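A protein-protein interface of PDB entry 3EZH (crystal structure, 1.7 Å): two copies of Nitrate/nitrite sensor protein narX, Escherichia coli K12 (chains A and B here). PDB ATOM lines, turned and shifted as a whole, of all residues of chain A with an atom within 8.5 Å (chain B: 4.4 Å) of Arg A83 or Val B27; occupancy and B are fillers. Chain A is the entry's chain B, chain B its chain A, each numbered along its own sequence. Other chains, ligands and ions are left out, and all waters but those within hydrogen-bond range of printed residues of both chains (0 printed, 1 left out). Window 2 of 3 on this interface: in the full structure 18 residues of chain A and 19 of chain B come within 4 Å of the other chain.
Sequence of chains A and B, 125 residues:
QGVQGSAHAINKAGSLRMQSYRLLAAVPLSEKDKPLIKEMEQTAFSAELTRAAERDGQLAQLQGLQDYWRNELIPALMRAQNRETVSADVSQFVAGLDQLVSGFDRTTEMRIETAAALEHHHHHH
Printed residues of chain A that touch a printed residue of chain B: Leu A24, Ala A25, Val A27 and Arg A83. Hydrophobic or aromatic side chains of chain A within 4 Å of the printed part of chain B: Leu A24 and Ala A25. Along chain A the printed residues that touch a printed residue of chain B span positions 24 to 83. Of the 12 printed residues of chain B, 4 touch a printed residue of chain A. Printed residues of chain B that touch a printed residue of chain A: Leu B24, Ala B25, Val B27 and Arg B83. Hydrophobic or aromatic side chains of chain B within 4 Å of the printed part of chain A: Leu B24 and Ala B25.
Among the printed residues, pairs that only touch across the chains: Leu A24 with Ala B25 (3.6 Å), Leu A24 with Arg B83 (3.9 Å), Ala A25 with Leu B24 (3.9 Å), Arg A83 with Leu B24 (3.96 Å) and Arg A83 with Arg B83 (3.5 Å).
Leu A24 touches Arg B83, and with the chains exchanged Arg A83 touches Leu B24. Ala A25 touches Arg B83, and with the chains exchanged Arg A83 touches Ala B25. Val A27 touches Arg B83, and with the chains exchanged Arg A83 touches Val B27. Arg B83 touches its own counterpart, Arg A83. Positions printed for both chains: 23, 24, 25, 26, 27, 28, 77, 80, 82, 83 and 86. Of the 9 pairs that touch across the chains among the printed residues, 9 have their exchanged pair printed and touching as well.
Arg A83 touches just these residues of chain B: Leu B24, Ala B25, Val B27 and Arg B83. No residue of chain A comes within 4 Å of Ala B26. Printed residues of chain A within 4 Å of Arg B83: Leu A24 (3.9 Å), Ala A25 (2.8 Å), Val A27 (2.8 Å) and Arg A83 (3.5 Å). Printed residues of chain B within 4 Å of Leu A24: Ala B25 (3.6 Å) and Arg B83 (3.9 Å). Of the printed residues of chain A, Leu B24 touches Ala A25 and Arg A83. Printed residues of chain B within 4 Å of Val A27: Arg B83 (2.8 Å). Of the printed residues of chain B, Ala A25 touches Leu B24 and Arg B83. The nearest residue of chain B that does not touch Arg A83 is Ala B26 (4.1 Å). The nearest printed residue of chain A that does not touch Ala B25 is Ala A25 (4.2 Å).
The backbone carbonyl oxygen (O) of Ala B25 sits at hydrogen-bond distance from the guanidinium group (NH1) of Arg A83, at 2.8 Å. NH1 of Arg B83 lies within hydrogen-bond range of O of Ala A25. The backbone carbonyl oxygen (O) of Val B27 sits at hydrogen-bond distance from the guanidinium group (NH1) of Arg A83 (2.7 Å). NH1 of Arg B83 sits at hydrogen-bond distance from O of Val A27 (2.8 Å).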
ATOM      1  N   TYR A  21      18.550  -9.443 -28.217  1.00  0.00           N
ATOM      2  CA  TYR A  21      18.147 -10.628 -28.917  1.00  0.00           C
ATOM      3  C   TYR A  21      19.168 -11.059 -29.957  1.00  0.00           C
ATOM      4  O   TYR A  21      19.155 -12.235 -30.359  1.00  0.00           O
ATOM      5  CB  TYR A  21      16.796 -10.392 -29.587  1.00  0.00           C
ATOM      6  CG  TYR A  21      15.627 -10.780 -28.686  1.00  0.00           C
ATOM      7  CD1 TYR A  21      15.340 -12.116 -28.488  1.00  0.00           C
ATOM      8  CD2 TYR A  21      14.843  -9.803 -28.084  1.00  0.00           C
ATOM      9  CE1 TYR A  21      14.268 -12.519 -27.679  1.00  0.00           C
ATOM     10  CE2 TYR A  21      13.721 -10.194 -27.251  1.00  0.00           C
ATOM     11  CZ  TYR A  21      13.476 -11.559 -27.085  1.00  0.00           C
ATOM     12  OH  TYR A  21      12.365 -11.984 -26.346  1.00  0.00           O
ATOM     13  N   LEU A  23      22.373 -10.939 -29.383  1.00  0.00           N
ATOM     14  CA  LEU A  23      23.264 -11.776 -28.584  1.00  0.00           C
ATOM     15  C   LEU A  23      22.600 -13.152 -28.321  1.00  0.00           C
ATOM     16  O   LEU A  23      23.260 -14.190 -28.396  1.00  0.00           O
ATOM     17  CB  LEU A  23      23.630 -11.053 -27.268  1.00  0.00           C
ATOM     18  CG  LEU A  23      24.783 -10.075 -27.400  1.00  0.00           C
ATOM     19  CD1 LEU A  23      24.873  -9.160 -26.148  1.00  0.00           C
ATOM     20  CD2 LEU A  23      26.063 -10.941 -27.524  1.00  0.00           C
ATOM     21  N   LEU A  24      21.290 -13.204 -28.027  1.00  0.00           N
ATOM     22  CA  LEU A  24      20.676 -14.503 -27.832  1.00  0.00           C
ATOM     23  C   LEU A  24      20.778 -15.336 -29.111  1.00  0.00           C
ATOM     24  O   LEU A  24      20.993 -16.547 -29.064  1.00  0.00           O
ATOM     25  CB  LEU A  24      19.167 -14.337 -27.426  1.00  0.00           C
ATOM     26  CG  LEU A  24      18.418 -15.641 -27.239  1.00  0.00           C
ATOM     27  CD1 LEU A  24      18.935 -16.377 -25.998  1.00  0.00           C
ATOM     28  CD2 LEU A  24      16.884 -15.310 -27.060  1.00  0.00           C
ATOM     29  N   ALA A  25      20.567 -14.694 -30.257  1.00  0.00           N
ATOM     30  CA  ALA A  25      20.601 -15.475 -31.498  1.00  0.00           C
ATOM     31  C   ALA A  25      22.021 -15.972 -31.800  1.00  0.00           C
ATOM     32  O   ALA A  25      22.217 -16.807 -32.701  1.00  0.00           O
ATOM     33  CB  ALA A  25      20.016 -14.640 -32.684  1.00  0.00           C
ATOM     34  N   ALA A  26      23.010 -15.468 -31.080  1.00  0.00           N
ATOM     35  CA  ALA A  26      24.415 -15.942 -31.316  1.00  0.00           C
ATOM     36  C   ALA A  26      24.850 -17.050 -30.342  1.00  0.00           C
ATOM     37  O   ALA A  26      25.991 -17.587 -30.436  1.00  0.00           O
ATOM     38  CB  ALA A  26      25.410 -14.741 -31.226  1.00  0.00           C
ATOM     39  N   VAL A  27      23.938 -17.445 -29.428  1.00  0.00           N
ATOM     40  CA  VAL A  27      24.301 -18.459 -28.414  1.00  0.00           C
ATOM     41  C   VAL A  27      24.471 -19.830 -29.050  1.00  0.00           C
ATOM     42  O   VAL A  27      23.664 -20.237 -29.876  1.00  0.00           O
ATOM     43  CB  VAL A  27      23.189 -18.497 -27.251  1.00  0.00           C
ATOM     44  CG1 VAL A  27      23.316 -19.781 -26.406  1.00  0.00           C
ATOM     45  CG2 VAL A  27      23.363 -17.239 -26.355  1.00  0.00           C
ATOM     46  N   PRO A  28      25.551 -20.566 -28.680  1.00  0.00           N
ATOM     47  CA  PRO A  28      26.640 -20.271 -27.745  1.00  0.00           C
ATOM     48  C   PRO A  28      27.602 -19.251 -28.319  1.00  0.00           C
ATOM     49  O   PRO A  28      28.067 -19.405 -29.452  1.00  0.00           O
ATOM     50  CB  PRO A  28      27.327 -21.645 -27.559  1.00  0.00           C
ATOM     51  CG  PRO A  28      27.184 -22.250 -28.887  1.00  0.00           C
ATOM     52  CD  PRO A  28      25.747 -21.896 -29.304  1.00  0.00           C
ATOM     53  N   ALA A  76      25.314 -14.579 -17.859  1.00  0.00           N
ATOM     54  CA  ALA A  76      24.442 -15.677 -18.236  1.00  0.00           C
ATOM     55  C   ALA A  76      24.489 -16.038 -19.700  1.00  0.00           C
ATOM     56  O   ALA A  76      24.437 -17.192 -20.061  1.00  0.00           O
ATOM     57  CB  ALA A  76      22.949 -15.348 -17.830  1.00  0.00           C
ATOM     58  N   LEU A  77      24.557 -15.029 -20.554  1.00  0.00           N
ATOM     59  CA  LEU A  77      24.621 -15.249 -22.005  1.00  0.00           C
ATOM     60  C   LEU A  77      25.979 -15.900 -22.364  1.00  0.00           C
ATOM     61  O   LEU A  77      26.021 -16.766 -23.249  1.00  0.00           O
ATOM     62  CB  LEU A  77      24.512 -13.914 -22.737  1.00  0.00           C
ATOM     63  CG  LEU A  77      23.076 -13.410 -22.995  1.00  0.00           C
ATOM     64  CD1 LEU A  77      23.084 -11.922 -23.339  1.00  0.00           C
ATOM     65  CD2 LEU A  77      22.446 -14.218 -24.104  1.00  0.00           C
ATOM     66  N   ALA A  80      25.960 -19.778 -21.430  1.00  0.00           N
ATOM     67  CA  ALA A  80      24.930 -20.628 -22.015  1.00  0.00           C
ATOM     68  C   ALA A  80      25.429 -21.470 -23.177  1.00  0.00           C
ATOM     69  O   ALA A  80      26.067 -20.956 -24.085  1.00  0.00           O
ATOM     70  CB  ALA A  80      23.763 -19.766 -22.485  1.00  0.00           C
ATOM     71  N   GLN A  81      25.111 -22.762 -23.161  1.00  0.00           N
ATOM     72  CA  GLN A  81      25.445 -23.637 -24.276  1.00  0.00           C
ATOM     73  C   GLN A  81      24.289 -23.641 -25.297  1.00  0.00           C
ATOM     74  O   GLN A  81      24.494 -23.878 -26.507  1.00  0.00           O
ATOM     75  CB  GLN A  81      25.648 -25.078 -23.809  1.00  0.00           C
ATOM     76  CG  GLN A  81      26.673 -25.325 -22.762  1.00  0.00           C
ATOM     77  CD  GLN A  81      26.745 -26.815 -22.506  1.00  0.00           C
ATOM     78  OE1 GLN A  81      27.546 -27.513 -23.118  1.00  0.00           O
ATOM     79  NE2 GLN A  81      25.864 -27.318 -21.632  1.00  0.00           N
ATOM     80  N   ASN A  82      23.057 -23.484 -24.784  1.00  0.00           N
ATOM     81  CA  ASN A  82      21.855 -23.426 -25.622  1.00  0.00           C
ATOM     82  C   ASN A  82      20.972 -22.239 -25.265  1.00  0.00           C
ATOM     83  O   ASN A  82      20.990 -21.780 -24.112  1.00  0.00           O
ATOM     84  CB  ASN A  82      20.995 -24.689 -25.515  1.00  0.00           C
ATOM     85  CG  ASN A  82      21.069 -25.327 -24.171  1.00  0.00           C
ATOM     86  OD1 ASN A  82      20.503 -24.821 -23.201  1.00  0.00           O
ATOM     87  ND2 ASN A  82      21.784 -26.456 -24.090  1.00  0.00           N
ATOM     88  N   ARG A  83      20.192 -21.794 -26.247  1.00  0.00           N
ATOM     89  CA  ARG A  83      19.313 -20.615 -26.066  1.00  0.00           C
ATOM     90  C   ARG A  83      18.293 -20.832 -24.927  1.00  0.00           C
ATOM     91  O   ARG A  83      17.985 -19.912 -24.183  1.00  0.00           O
ATOM     92  CB  ARG A  83      18.582 -20.374 -27.390  1.00  0.00           C
ATOM     93  CG  ARG A  83      19.517 -19.755 -28.451  1.00  0.00           C
ATOM     94  CD  ARG A  83      18.735 -19.710 -29.762  1.00  0.00           C
ATOM     95  NE  ARG A  83      18.708 -21.038 -30.364  1.00  0.00           N
ATOM     96  CZ  ARG A  83      18.010 -21.380 -31.444  1.00  0.00           C
ATOM     97  NH1 ARG A  83      17.204 -20.501 -32.069  1.00  0.00           N
ATOM     98  NH2 ARG A  83      18.197 -22.594 -31.955  1.00  0.00           N
ATOM     99  N   GLU A  84      17.819 -22.067 -24.789  1.00  0.00           N
ATOM    100  CA  GLU A  84      16.773 -22.385 -23.801  1.00  0.00           C
ATOM    101  C   GLU A  84      17.076 -22.019 -22.348  1.00  0.00           C
ATOM    102  O   GLU A  84      16.157 -21.667 -21.605  1.00  0.00           O
ATOM    103  CB  GLU A  84      16.404 -23.879 -23.917  1.00  0.00           C
ATOM    104  CG  GLU A  84      17.026 -24.498 -25.161  1.00  0.00           C
ATOM    105  CD  GLU A  84      16.573 -25.911 -25.415  1.00  0.00           C
ATOM    106  OE1 GLU A  84      16.757 -26.767 -24.513  1.00  0.00           O
ATOM    107  OE2 GLU A  84      16.040 -26.154 -26.525  1.00  0.00           O
ATOM    108  N   THR A  85      18.334 -22.055 -21.937  1.00  0.00           N
ATOM    109  CA  THR A  85      18.662 -21.718 -20.550  1.00  0.00           C
ATOM    110  C   THR A  85      18.696 -20.233 -20.217  1.00  0.00           C
ATOM    111  O   THR A  85      18.691 -19.862 -19.034  1.00  0.00           O
ATOM    112  CB  THR A  85      20.018 -22.327 -20.059  1.00  0.00           C
ATOM    113  OG1 THR A  85      21.107 -21.777 -20.800  1.00  0.00           O
ATOM    114  CG2 THR A  85      20.028 -23.833 -20.272  1.00  0.00           C
ATOM    115  N   VAL A  86      18.671 -19.377 -21.235  1.00  0.00           N
ATOM    116  CA  VAL A  86      18.784 -17.945 -21.010  1.00  0.00           C
ATOM    117  C   VAL A  86      17.767 -17.135 -21.843  1.00  0.00           C
ATOM    118  O   VAL A  86      17.696 -15.954 -21.705  1.00  0.00           O
ATOM    119  CB  VAL A  86      20.280 -17.490 -21.309  1.00  0.00           C
ATOM    120  CG1 VAL A  86      20.594 -17.712 -22.795  1.00  0.00           C
ATOM    121  CG2 VAL A  86      20.556 -16.052 -20.865  1.00  0.00           C
ATOM    122  N   SER A  87      16.967 -17.771 -22.683  1.00  0.00           N
ATOM    123  CA  SER A  87      15.990 -17.021 -23.466  1.00  0.00           C
ATOM    124  C   SER A  87      14.944 -16.266 -22.623  1.00  0.00           C
ATOM    125  O   SER A  87      14.641 -15.120 -22.955  1.00  0.00           O
ATOM    126  CB  SER A  87      15.314 -17.914 -24.493  1.00  0.00           C
ATOM    127  OG  SER A  87      14.541 -18.982 -23.920  1.00  0.00           O
ATOM    128  N   ALA A  88      14.396 -16.872 -21.550  1.00  0.00           N
ATOM    129  CA  ALA A  88      13.454 -16.111 -20.756  1.00  0.00           C
ATOM    130  C   ALA A  88      14.084 -14.865 -20.090  1.00  0.00           C
ATOM    131  O   ALA A  88      13.450 -13.800 -20.023  1.00  0.00           O
ATOM    132  CB  ALA A  88      12.787 -17.044 -19.713  1.00  0.00           C
ATOM    133  N   ASP A  89      15.335 -14.979 -19.642  1.00  0.00           N
ATOM    134  CA  ASP A  89      16.084 -13.896 -19.016  1.00  0.00           C
ATOM    135  C   ASP A  89      16.255 -12.790 -20.035  1.00  0.00           C
ATOM    136  O   ASP A  89      16.119 -11.639 -19.737  1.00  0.00           O
ATOM    137  CB  ASP A  89      17.441 -14.422 -18.569  1.00  0.00           C
ATOM    138  CG  ASP A  89      18.168 -13.492 -17.588  1.00  0.00           C
ATOM    139  OD1 ASP A  89      17.562 -12.667 -16.864  1.00  0.00           O
ATOM    140  OD2 ASP A  89      19.420 -13.619 -17.511  1.00  0.00           O
ATOM    141  N   VAL A  90      16.569 -13.161 -21.269  1.00  0.00           N
ATOM    142  CA  VAL A  90      16.686 -12.096 -22.296  1.00  0.00           C
ATOM    143  C   VAL A  90      15.358 -11.347 -22.554  1.00  0.00           C
ATOM    144  O   VAL A  90      15.328 -10.100 -22.623  1.00  0.00           O
ATOM    145  CB  VAL A  90      17.183 -12.685 -23.610  1.00  0.00           C
ATOM    146  CG1 VAL A  90      17.159 -11.623 -24.737  1.00  0.00           C
ATOM    147  CG2 VAL A  90      18.684 -13.155 -23.405  1.00  0.00           C
ATOM    148  N   LEU B  23      12.491 -13.262 -33.704  1.00  0.00           N
ATOM    149  CA  LEU B  23      12.090 -14.397 -34.514  1.00  0.00           C
ATOM    150  C   LEU B  23      13.331 -15.244 -34.870  1.00  0.00           C
ATOM    151  O   LEU B  23      13.269 -16.440 -34.925  1.00  0.00           O
ATOM    152  CB  LEU B  23      11.398 -13.896 -35.790  1.00  0.00           C
ATOM    153  CG  LEU B  23       9.923 -13.526 -35.621  1.00  0.00           C
ATOM    154  CD1 LEU B  23       9.316 -12.816 -36.859  1.00  0.00           C
ATOM    155  CD2 LEU B  23       9.131 -14.846 -35.411  1.00  0.00           C
ATOM    156  N   LEU B  24      14.473 -14.594 -35.123  1.00  0.00           N
ATOM    157  CA  LEU B  24      15.678 -15.386 -35.438  1.00  0.00           C
ATOM    158  C   LEU B  24      16.043 -16.276 -34.259  1.00  0.00           C
ATOM    159  O   LEU B  24      16.404 -17.429 -34.431  1.00  0.00           O
ATOM    160  CB  LEU B  24      16.846 -14.463 -35.810  1.00  0.00           C
ATOM    161  CG  LEU B  24      18.104 -15.298 -36.251  1.00  0.00           C
ATOM    162  CD1 LEU B  24      17.851 -16.085 -37.554  1.00  0.00           C
ATOM    163  CD2 LEU B  24      19.243 -14.334 -36.457  1.00  0.00           C
ATOM    164  N   ALA B  25      16.010 -15.703 -33.053  1.00  0.00           N
ATOM    165  CA  ALA B  25      16.328 -16.470 -31.850  1.00  0.00           C
ATOM    166  C   ALA B  25      15.376 -17.624 -31.627  1.00  0.00           C
ATOM    167  O   ALA B  25      15.687 -18.507 -30.820  1.00  0.00           O
ATOM    168  CB  ALA B  25      16.310 -15.567 -30.642  1.00  0.00           C
ATOM    169  N   ALA B  26      14.220 -17.642 -32.277  1.00  0.00           N
ATOM    170  CA  ALA B  26      13.250 -18.738 -32.095  1.00  0.00           C
ATOM    171  C   ALA B  26      13.293 -19.805 -33.174  1.00  0.00           C
ATOM    172  O   ALA B  26      12.512 -20.778 -33.136  1.00  0.00           O
ATOM    173  CB  ALA B  26      11.810 -18.180 -31.997  1.00  0.00           C
ATOM    174  N   VAL B  27      14.219 -19.626 -34.129  1.00  0.00           N
ATOM    175  CA  VAL B  27      14.398 -20.560 -35.216  1.00  0.00           C
ATOM    176  C   VAL B  27      14.968 -21.902 -34.712  1.00  0.00           C
ATOM    177  O   VAL B  27      15.923 -21.915 -33.958  1.00  0.00           O
ATOM    178  CB  VAL B  27      15.394 -19.990 -36.267  1.00  0.00           C
ATOM    179  CG1 VAL B  27      15.807 -21.121 -37.247  1.00  0.00           C
ATOM    180  CG2 VAL B  27      14.678 -18.903 -37.072  1.00  0.00           C
ATOM    181  N   PRO B  28      14.402 -23.034 -35.156  1.00  0.00           N
ATOM    182  CA  PRO B  28      13.275 -23.217 -36.080  1.00  0.00           C
ATOM    183  C   PRO B  28      11.901 -22.905 -35.469  1.00  0.00           C
ATOM    184  O   PRO B  28      11.549 -23.346 -34.351  1.00  0.00           O
ATOM    185  CB  PRO B  28      13.414 -24.686 -36.517  1.00  0.00           C
ATOM    186  CG  PRO B  28      14.004 -25.335 -35.371  1.00  0.00           C
ATOM    187  CD  PRO B  28      15.004 -24.340 -34.816  1.00  0.00           C
ATOM    188  N   LEU B  29      11.118 -22.163 -36.243  1.00  0.00           N
ATOM    189  CA  LEU B  29       9.788 -21.723 -35.812  1.00  0.00           C
ATOM    190  C   LEU B  29       8.755 -22.833 -35.756  1.00  0.00           C
ATOM    191  O   LEU B  29       8.777 -23.763 -36.560  1.00  0.00           O
ATOM    192  CB  LEU B  29       9.241 -20.630 -36.754  1.00  0.00           C
ATOM    193  CG  LEU B  29      10.145 -19.410 -36.970  1.00  0.00           C
ATOM    194  CD1 LEU B  29       9.403 -18.358 -37.825  1.00  0.00           C
ATOM    195  CD2 LEU B  29      10.561 -18.764 -35.646  1.00  0.00           C
ATOM    196  N   LEU B  77      12.153 -17.256 -42.985  1.00  0.00           N
ATOM    197  CA  LEU B  77      12.206 -17.547 -41.578  1.00  0.00           C
ATOM    198  C   LEU B  77      11.359 -18.783 -41.250  1.00  0.00           C
ATOM    199  O   LEU B  77      11.754 -19.597 -40.426  1.00  0.00           O
ATOM    200  CB  LEU B  77      11.741 -16.328 -40.772  1.00  0.00           C
ATOM    201  CG  LEU B  77      12.798 -15.237 -40.492  1.00  0.00           C
ATOM    202  CD1 LEU B  77      12.065 -13.966 -40.040  1.00  0.00           C
ATOM    203  CD2 LEU B  77      13.824 -15.652 -39.403  1.00  0.00           C
ATOM    204  N   ALA B  80      13.325 -21.965 -42.551  1.00  0.00           N
ATOM    205  CA  ALA B  80      14.600 -22.239 -41.896  1.00  0.00           C
ATOM    206  C   ALA B  80      14.636 -23.366 -40.875  1.00  0.00           C
ATOM    207  O   ALA B  80      13.876 -23.366 -39.907  1.00  0.00           O
ATOM    208  CB  ALA B  80      15.162 -20.954 -41.238  1.00  0.00           C
ATOM    209  N   ASN B  82      17.584 -23.953 -39.419  1.00  0.00           N
ATOM    210  CA  ASN B  82      18.654 -23.531 -38.509  1.00  0.00           C
ATOM    211  C   ASN B  82      18.928 -22.011 -38.703  1.00  0.00           C
ATOM    212  O   ASN B  82      18.528 -21.435 -39.729  1.00  0.00           O
ATOM    213  CB  ASN B  82      19.911 -24.384 -38.683  1.00  0.00           C
ATOM    214  CG  ASN B  82      20.520 -24.265 -40.047  1.00  0.00           C
ATOM    215  OD1 ASN B  82      21.018 -25.255 -40.595  1.00  0.00           O
ATOM    216  ND2 ASN B  82      20.512 -23.064 -40.608  1.00  0.00           N
ATOM    217  N   ARG B  83      19.497 -21.366 -37.703  1.00  0.00           N
ATOM    218  CA  ARG B  83      19.718 -19.915 -37.754  1.00  0.00           C
ATOM    219  C   ARG B  83      20.609 -19.420 -38.889  1.00  0.00           C
ATOM    220  O   ARG B  83      20.410 -18.335 -39.404  1.00  0.00           O
ATOM    221  CB  ARG B  83      20.290 -19.432 -36.422  1.00  0.00           C
ATOM    222  CG  ARG B  83      19.206 -19.428 -35.260  1.00  0.00           C
ATOM    223  CD  ARG B  83      19.889 -19.203 -33.931  1.00  0.00           C
ATOM    224  NE  ARG B  83      20.634 -20.402 -33.512  1.00  0.00           N
ATOM    225  CZ  ARG B  83      21.454 -20.443 -32.450  1.00  0.00           C
ATOM    226  NH1 ARG B  83      21.675 -19.362 -31.704  1.00  0.00           N
ATOM    227  NH2 ARG B  83      21.998 -21.601 -32.089  1.00  0.00           N
ATOM    228  N   VAL B  86      19.296 -18.098 -42.265  1.00  0.00           N
ATOM    229  CA  VAL B  86      18.591 -16.841 -42.377  1.00  0.00           C
ATOM    230  C   VAL B  86      19.236 -15.713 -41.609  1.00  0.00           C
ATOM    231  O   VAL B  86      18.745 -14.583 -41.644  1.00  0.00           O
ATOM    232  CB  VAL B  86      17.123 -16.991 -41.913  1.00  0.00           C
ATOM    233  CG1 VAL B  86      16.336 -17.692 -42.976  1.00  0.00           C
ATOM    234  CG2 VAL B  86      17.052 -17.805 -40.579  1.00  0.00           C
